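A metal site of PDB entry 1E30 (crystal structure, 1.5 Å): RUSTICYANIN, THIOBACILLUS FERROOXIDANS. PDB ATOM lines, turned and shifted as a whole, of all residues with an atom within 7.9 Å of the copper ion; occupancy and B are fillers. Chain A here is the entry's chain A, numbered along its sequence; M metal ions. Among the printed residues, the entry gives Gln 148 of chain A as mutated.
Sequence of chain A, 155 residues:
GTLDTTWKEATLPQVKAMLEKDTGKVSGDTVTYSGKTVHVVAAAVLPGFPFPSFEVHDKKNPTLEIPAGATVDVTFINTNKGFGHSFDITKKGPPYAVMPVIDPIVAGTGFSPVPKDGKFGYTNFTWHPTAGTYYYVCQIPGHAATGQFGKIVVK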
ATOM      1  N   ALA A  44     -22.535 -14.510  20.762  1.00  0.00           N
ATOM      2  CA  ALA A  44     -23.607 -15.303  21.353  1.00  0.00           C
ATOM      3  C   ALA A  44     -23.252 -16.753  21.106  1.00  0.00           C
ATOM      4  O   ALA A  44     -23.177 -17.147  19.929  1.00  0.00           O
ATOM      5  CB  ALA A  44     -24.919 -14.917  20.694  1.00  0.00           C
ATOM      6  N   VAL A  45     -22.968 -17.520  22.110  1.00  0.00           N
ATOM      7  CA  VAL A  45     -22.654 -18.933  22.112  1.00  0.00           C
ATOM      8  C   VAL A  45     -21.549 -19.358  21.148  1.00  0.00           C
ATOM      9  O   VAL A  45     -21.714 -19.847  20.043  1.00  0.00           O
ATOM     10  CB  VAL A  45     -23.913 -19.794  21.821  1.00  0.00           C
ATOM     11  CG1 VAL A  45     -23.603 -21.251  22.126  1.00  0.00           C
ATOM     12  CG2 VAL A  45     -25.092 -19.344  22.655  1.00  0.00           C
ATOM     13  N   PHE A  51     -25.306 -22.946  25.864  1.00  0.00           N
ATOM     14  CA  PHE A  51     -26.447 -22.234  25.313  1.00  0.00           C
ATOM     15  C   PHE A  51     -27.475 -21.967  26.399  1.00  0.00           C
ATOM     16  O   PHE A  51     -27.792 -22.852  27.188  1.00  0.00           O
ATOM     17  CB  PHE A  51     -27.089 -23.133  24.234  1.00  0.00           C
ATOM     18  CG  PHE A  51     -28.376 -22.552  23.692  1.00  0.00           C
ATOM     19  CD1 PHE A  51     -29.577 -22.760  24.359  1.00  0.00           C
ATOM     20  CD2 PHE A  51     -28.374 -21.792  22.548  1.00  0.00           C
ATOM     21  CE1 PHE A  51     -30.741 -22.227  23.861  1.00  0.00           C
ATOM     22  CE2 PHE A  51     -29.521 -21.252  22.037  1.00  0.00           C
ATOM     23  CZ  PHE A  51     -30.733 -21.464  22.695  1.00  0.00           C
ATOM     24  N   PRO A  52     -28.044 -20.778  26.431  1.00  0.00           N
ATOM     25  CA  PRO A  52     -27.670 -19.620  25.646  1.00  0.00           C
ATOM     26  C   PRO A  52     -26.782 -18.725  26.500  1.00  0.00           C
ATOM     27  O   PRO A  52     -27.029 -18.573  27.690  1.00  0.00           O
ATOM     28  CB  PRO A  52     -29.032 -18.968  25.414  1.00  0.00           C
ATOM     29  CG  PRO A  52     -29.834 -19.295  26.637  1.00  0.00           C
ATOM     30  CD  PRO A  52     -29.165 -20.431  27.377  1.00  0.00           C
ATOM     31  N   SER A  53     -25.691 -18.187  25.979  1.00  0.00           N
ATOM     32  CA  SER A  53     -24.789 -17.361  26.773  1.00  0.00           C
ATOM     33  C   SER A  53     -24.072 -16.413  25.828  1.00  0.00           C
ATOM     34  O   SER A  53     -24.139 -16.591  24.626  1.00  0.00           O
ATOM     35  CB  SER A  53     -23.698 -18.202  27.455  1.00  0.00           C
ATOM     36  OG  SER A  53     -22.881 -18.882  26.526  1.00  0.00           O
ATOM     37  N   PHE A  54     -23.485 -15.402  26.456  1.00  0.00           N
ATOM     38  CA  PHE A  54     -22.642 -14.484  25.711  1.00  0.00           C
ATOM     39  C   PHE A  54     -21.184 -14.727  26.109  1.00  0.00           C
ATOM     40  O   PHE A  54     -20.955 -14.982  27.285  1.00  0.00           O
ATOM     41  CB  PHE A  54     -22.906 -13.033  26.087  1.00  0.00           C
ATOM     42  CG  PHE A  54     -24.226 -12.457  25.676  1.00  0.00           C
ATOM     43  CD1 PHE A  54     -24.511 -12.220  24.337  1.00  0.00           C
ATOM     44  CD2 PHE A  54     -25.132 -12.094  26.657  1.00  0.00           C
ATOM     45  CE1 PHE A  54     -25.737 -11.670  23.968  1.00  0.00           C
ATOM     46  CE2 PHE A  54     -26.348 -11.557  26.285  1.00  0.00           C
ATOM     47  CZ  PHE A  54     -26.620 -11.325  24.944  1.00  0.00           C
ATOM     48  N   PHE A  76     -21.032  -7.021  18.421  1.00  0.00           N
ATOM     49  CA  PHE A  76     -21.814  -8.190  18.801  1.00  0.00           C
ATOM     50  C   PHE A  76     -21.877  -9.130  17.609  1.00  0.00           C
ATOM     51  O   PHE A  76     -22.252  -8.702  16.513  1.00  0.00           O
ATOM     52  CB  PHE A  76     -23.223  -7.818  19.267  1.00  0.00           C
ATOM     53  CG  PHE A  76     -24.100  -9.017  19.504  1.00  0.00           C
ATOM     54  CD1 PHE A  76     -23.701 -10.038  20.358  1.00  0.00           C
ATOM     55  CD2 PHE A  76     -25.281  -9.158  18.805  1.00  0.00           C
ATOM     56  CE1 PHE A  76     -24.481 -11.169  20.565  1.00  0.00           C
ATOM     57  CE2 PHE A  76     -26.091 -10.260  18.983  1.00  0.00           C
ATOM     58  CZ  PHE A  76     -25.680 -11.238  19.869  1.00  0.00           C
ATOM     59  N   ASN A  78     -23.164 -12.911  16.206  1.00  0.00           N
ATOM     60  CA  ASN A  78     -23.988 -14.087  16.498  1.00  0.00           C
ATOM     61  C   ASN A  78     -23.303 -15.282  15.843  1.00  0.00           C
ATOM     62  O   ASN A  78     -23.425 -15.529  14.656  1.00  0.00           O
ATOM     63  CB  ASN A  78     -25.436 -13.874  16.020  1.00  0.00           C
ATOM     64  CG  ASN A  78     -26.254 -15.122  16.272  1.00  0.00           C
ATOM     65  OD1 ASN A  78     -27.365 -15.323  15.717  1.00  0.00           O
ATOM     66  ND2 ASN A  78     -25.778 -16.042  17.076  1.00  0.00           N
ATOM     67  N   ASN A  80     -24.030 -18.359  16.835  1.00  0.00           N
ATOM     68  CA  ASN A  80     -24.810 -19.554  17.179  1.00  0.00           C
ATOM     69  C   ASN A  80     -25.707 -20.068  16.066  1.00  0.00           C
ATOM     70  O   ASN A  80     -26.784 -19.575  15.789  1.00  0.00           O
ATOM     71  CB  ASN A  80     -25.581 -19.269  18.465  1.00  0.00           C
ATOM     72  CG  ASN A  80     -26.252 -20.417  19.144  1.00  0.00           C
ATOM     73  OD1 ASN A  80     -25.794 -21.581  19.056  1.00  0.00           O
ATOM     74  ND2 ASN A  80     -27.294 -20.122  19.888  1.00  0.00           N
ATOM     75  N   PHE A  83     -29.899 -20.013  15.545  1.00  0.00           N
ATOM     76  CA  PHE A  83     -30.577 -19.151  16.491  1.00  0.00           C
ATOM     77  C   PHE A  83     -30.294 -17.670  16.249  1.00  0.00           C
ATOM     78  O   PHE A  83     -29.150 -17.327  15.965  1.00  0.00           O
ATOM     79  CB  PHE A  83     -30.073 -19.420  17.926  1.00  0.00           C
ATOM     80  CG  PHE A  83     -30.566 -20.738  18.458  1.00  0.00           C
ATOM     81  CD1 PHE A  83     -31.803 -20.820  19.068  1.00  0.00           C
ATOM     82  CD2 PHE A  83     -29.768 -21.858  18.349  1.00  0.00           C
ATOM     83  CE1 PHE A  83     -32.255 -22.036  19.558  1.00  0.00           C
ATOM     84  CE2 PHE A  83     -30.214 -23.075  18.832  1.00  0.00           C
ATOM     85  CZ  PHE A  83     -31.457 -23.149  19.422  1.00  0.00           C
ATOM     86  N   GLY A  84     -31.317 -16.878  16.455  1.00  0.00           N
ATOM     87  CA  GLY A  84     -31.111 -15.422  16.412  1.00  0.00           C
ATOM     88  C   GLY A  84     -30.851 -15.075  17.889  1.00  0.00           C
ATOM     89  O   GLY A  84     -31.169 -15.807  18.830  1.00  0.00           O
ATOM     90  N   HIS A  85     -30.096 -14.013  18.088  1.00  0.00           N
ATOM     91  CA  HIS A  85     -29.806 -13.504  19.427  1.00  0.00           C
ATOM     92  C   HIS A  85     -29.744 -11.988  19.323  1.00  0.00           C
ATOM     93  O   HIS A  85     -29.549 -11.438  18.233  1.00  0.00           O
ATOM     94  CB  HIS A  85     -28.438 -13.972  19.906  1.00  0.00           C
ATOM     95  CG  HIS A  85     -28.416 -15.422  20.256  1.00  0.00           C
ATOM     96  ND1 HIS A  85     -29.076 -15.972  21.336  1.00  0.00           N
ATOM     97  CD2 HIS A  85     -27.800 -16.461  19.618  1.00  0.00           C
ATOM     98  CE1 HIS A  85     -28.827 -17.268  21.375  1.00  0.00           C
ATOM     99  NE2 HIS A  85     -28.079 -17.588  20.335  1.00  0.00           N
ATOM    100  N   SER A  86     -29.941 -11.307  20.417  1.00  0.00           N
ATOM    101  CA  SER A  86     -29.799  -9.861  20.440  1.00  0.00           C
ATOM    102  C   SER A  86     -28.810  -9.528  21.559  1.00  0.00           C
ATOM    103  O   SER A  86     -28.434 -10.381  22.388  1.00  0.00           O
ATOM    104  CB  SER A  86     -31.133  -9.162  20.632  1.00  0.00           C
ATOM    105  OG  SER A  86     -31.490  -9.219  22.016  1.00  0.00           O
ATOM    106  N   PHE A  87     -28.396  -8.272  21.595  1.00  0.00           N
ATOM    107  CA  PHE A  87     -27.499  -7.777  22.646  1.00  0.00           C
ATOM    108  C   PHE A  87     -27.981  -6.379  23.015  1.00  0.00           C
ATOM    109  O   PHE A  87     -27.856  -5.440  22.229  1.00  0.00           O
ATOM    110  CB  PHE A  87     -26.058  -7.719  22.170  1.00  0.00           C
ATOM    111  CG  PHE A  87     -25.020  -7.306  23.191  1.00  0.00           C
ATOM    112  CD1 PHE A  87     -24.847  -5.985  23.568  1.00  0.00           C
ATOM    113  CD2 PHE A  87     -24.206  -8.283  23.747  1.00  0.00           C
ATOM    114  CE1 PHE A  87     -23.910  -5.661  24.527  1.00  0.00           C
ATOM    115  CE2 PHE A  87     -23.249  -7.940  24.681  1.00  0.00           C
ATOM    116  CZ  PHE A  87     -23.089  -6.640  25.075  1.00  0.00           C
ATOM    117  N   SER A 112     -30.796 -10.581  15.743  1.00  0.00           N
ATOM    118  CA  SER A 112     -29.896 -10.828  14.600  1.00  0.00           C
ATOM    119  C   SER A 112     -30.470 -11.873  13.659  1.00  0.00           C
ATOM    120  O   SER A 112     -31.310 -12.684  14.015  1.00  0.00           O
ATOM    121  CB  SER A 112     -28.579 -11.407  15.127  1.00  0.00           C
ATOM    122  OG  SER A 112     -28.743 -12.762  15.533  1.00  0.00           O
ATOM    123  N   VAL A 137     -28.261  -8.063  27.801  1.00  0.00           N
ATOM    124  CA  VAL A 137     -29.198  -9.180  27.782  1.00  0.00           C
ATOM    125  C   VAL A 137     -29.702  -9.514  26.388  1.00  0.00           C
ATOM    126  O   VAL A 137     -29.725  -8.641  25.525  1.00  0.00           O
ATOM    127  CB  VAL A 137     -30.282  -9.118  28.857  1.00  0.00           C
ATOM    128  CG1 VAL A 137     -30.196  -7.958  29.861  1.00  0.00           C
ATOM    129  CG2 VAL A 137     -31.734  -9.361  28.505  1.00  0.00           C
ATOM    130  N   CYS A 138     -30.013 -10.800  26.154  1.00  0.00           N
ATOM    131  CA  CYS A 138     -30.641 -11.155  24.881  1.00  0.00           C
ATOM    132  C   CYS A 138     -32.162 -11.092  25.053  1.00  0.00           C
ATOM    133  O   CYS A 138     -32.673 -11.533  26.075  1.00  0.00           O
ATOM    134  CB  CYS A 138     -30.246 -12.586  24.521  1.00  0.00           C
ATOM    135  SG  CYS A 138     -31.061 -13.086  22.951  1.00  0.00           S
ATOM    136  N   GLN A 139     -32.859 -10.573  24.031  1.00  0.00           N
ATOM    137  CA  GLN A 139     -34.301 -10.431  24.103  1.00  0.00           C
ATOM    138  C   GLN A 139     -35.064 -11.540  23.392  1.00  0.00           C
ATOM    139  O   GLN A 139     -36.281 -11.497  23.361  1.00  0.00           O
ATOM    140  CB  GLN A 139     -34.739  -9.072  23.532  1.00  0.00           C
ATOM    141  CG  GLN A 139     -34.304  -7.881  24.366  1.00  0.00           C
ATOM    142  CD  GLN A 139     -35.230  -6.717  24.009  1.00  0.00           C
ATOM    143  OE1 GLN A 139     -35.060  -6.137  22.935  1.00  0.00           O
ATOM    144  NE2 GLN A 139     -36.195  -6.413  24.869  1.00  0.00           N
ATOM    145  N   ILE A 140     -34.350 -12.493  22.786  1.00  0.00           N
ATOM    146  CA  ILE A 140     -35.098 -13.594  22.112  1.00  0.00           C
ATOM    147  C   ILE A 140     -35.840 -14.295  23.232  1.00  0.00           C
ATOM    148  O   ILE A 140     -35.256 -14.572  24.263  1.00  0.00           O
ATOM    149  CB  ILE A 140     -34.116 -14.570  21.473  1.00  0.00           C
ATOM    150  CG1 ILE A 140     -33.385 -13.870  20.331  1.00  0.00           C
ATOM    151  CG2 ILE A 140     -34.829 -15.835  20.977  1.00  0.00           C
ATOM    152  CD1 ILE A 140     -34.195 -13.455  19.135  1.00  0.00           C
ATOM    153  N   PRO A 141     -37.150 -14.493  23.112  1.00  0.00           N
ATOM    154  CA  PRO A 141     -37.913 -15.080  24.201  1.00  0.00           C
ATOM    155  C   PRO A 141     -37.278 -16.305  24.805  1.00  0.00           C
ATOM    156  O   PRO A 141     -36.863 -17.269  24.147  1.00  0.00           O
ATOM    157  CB  PRO A 141     -39.273 -15.344  23.536  1.00  0.00           C
ATOM    158  CG  PRO A 141     -39.365 -14.201  22.571  1.00  0.00           C
ATOM    159  CD  PRO A 141     -37.976 -14.111  21.945  1.00  0.00           C
ATOM    160  N   GLY A 142     -37.134 -16.284  26.128  1.00  0.00           N
ATOM    161  CA  GLY A 142     -36.617 -17.343  26.942  1.00  0.00           C
ATOM    162  C   GLY A 142     -35.121 -17.336  27.187  1.00  0.00           C
ATOM    163  O   GLY A 142     -34.696 -17.924  28.171  1.00  0.00           O
ATOM    164  N   HIS A 143     -34.356 -16.641  26.348  1.00  0.00           N
ATOM    165  CA  HIS A 143     -32.888 -16.700  26.498  1.00  0.00           C
ATOM    166  C   HIS A 143     -32.361 -16.057  27.746  1.00  0.00           C
ATOM    167  O   HIS A 143     -31.492 -16.624  28.433  1.00  0.00           O
ATOM    168  CB  HIS A 143     -32.283 -16.058  25.245  1.00  0.00           C
ATOM    169  CG  HIS A 143     -32.438 -16.855  23.973  1.00  0.00           C
ATOM    170  ND1 HIS A 143     -31.698 -16.603  22.850  1.00  0.00           N
ATOM    171  CD2 HIS A 143     -33.305 -17.886  23.689  1.00  0.00           C
ATOM    172  CE1 HIS A 143     -32.068 -17.468  21.916  1.00  0.00           C
ATOM    173  NE2 HIS A 143     -33.036 -18.252  22.383  1.00  0.00           N
ATOM    174  N   ALA A 144     -32.846 -14.838  28.081  1.00  0.00           N
ATOM    175  CA  ALA A 144     -32.389 -14.192  29.295  1.00  0.00           C
ATOM    176  C   ALA A 144     -32.889 -14.967  30.508  1.00  0.00           C
ATOM    177  O   ALA A 144     -32.155 -15.146  31.470  1.00  0.00           O
ATOM    178  CB  ALA A 144     -32.886 -12.761  29.295  1.00  0.00           C
ATOM    179  N   THR A 146     -33.097 -18.027  30.741  1.00  0.00           N
ATOM    180  CA  THR A 146     -32.251 -19.207  30.914  1.00  0.00           C
ATOM    181  C   THR A 146     -30.774 -18.859  31.000  1.00  0.00           C
ATOM    182  O   THR A 146     -29.906 -19.721  30.789  1.00  0.00           O
ATOM    183  CB  THR A 146     -32.536 -20.274  29.851  1.00  0.00           C
ATOM    184  OG1 THR A 146     -32.380 -19.687  28.568  1.00  0.00           O
ATOM    185  CG2 THR A 146     -33.944 -20.854  29.993  1.00  0.00           C
ATOM    186  N   GLN A 148     -28.897 -15.967  29.513  1.00  0.00           N
ATOM    187  CA  GLN A 148     -28.102 -15.193  28.561  1.00  0.00           C
ATOM    188  C   GLN A 148     -28.142 -13.700  28.897  1.00  0.00           C
ATOM    189  O   GLN A 148     -28.881 -12.908  28.347  1.00  0.00           O
ATOM    190  CB  GLN A 148     -28.584 -15.418  27.134  1.00  0.00           C
ATOM    191  CG  GLN A 148     -27.601 -14.815  26.122  1.00  0.00           C
ATOM    192  CD  GLN A 148     -27.994 -15.167  24.707  1.00  0.00           C
ATOM    193  OE1 GLN A 148     -29.098 -15.656  24.491  1.00  0.00           O
ATOM    194  NE2 GLN A 148     -27.094 -14.932  23.771  1.00  0.00           N
HETATM  195 CU    CU M   1     -30.383 -15.131  22.621  1.00  0.00          CU
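The copper ion is bound by ND1 of His 143 (2.0 Å), ND1 of His 85 (2.0 Å), SG of Cys 138 (2.2 Å) and OE1 of Gln 148 (2.3 Å).
The copper ion has four donor atoms within binding distance.
Residues that only touch the copper ion: Gly 84 (3.9 Å) and Ile 140 (3.9 Å).
Six residues have an atom within 4 Å of the copper ion: Gly 84, His 85, Cys 138, Ile 140, His 143 and Gln 148.
Along chain A the residues within 4 Å of the copper ion span positions 84 to 148.
The nearest printed residue that does not touch the copper ion is Ser 86 (4.4 Å).
O of His 143 lies within hydrogen-bond range of OG1 of Thr 146 (3.2 Å).
ND2 of Asn 80 sits at hydrogen-bond distance from NE2 of His 85, at 2.7 Å.
The backbone carbonyl oxygen of His 85 sits at hydrogen-bond distance from the backbone NH of Ser 112 (2.9 Å).
The side-chain sulfur (SG) of Cys 138 sits close to the backbone NH (N) of Ile 140 (3.3 Å).
SG of Cys 138 sits close to N of Ser 86, 3.3 Å away.
The backbone carbonyl oxygen (O) of Ser 53 is in hydrogen-bond range of the side-chain amide nitrogen (NE2) of Gln 148 (3.5 Å).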
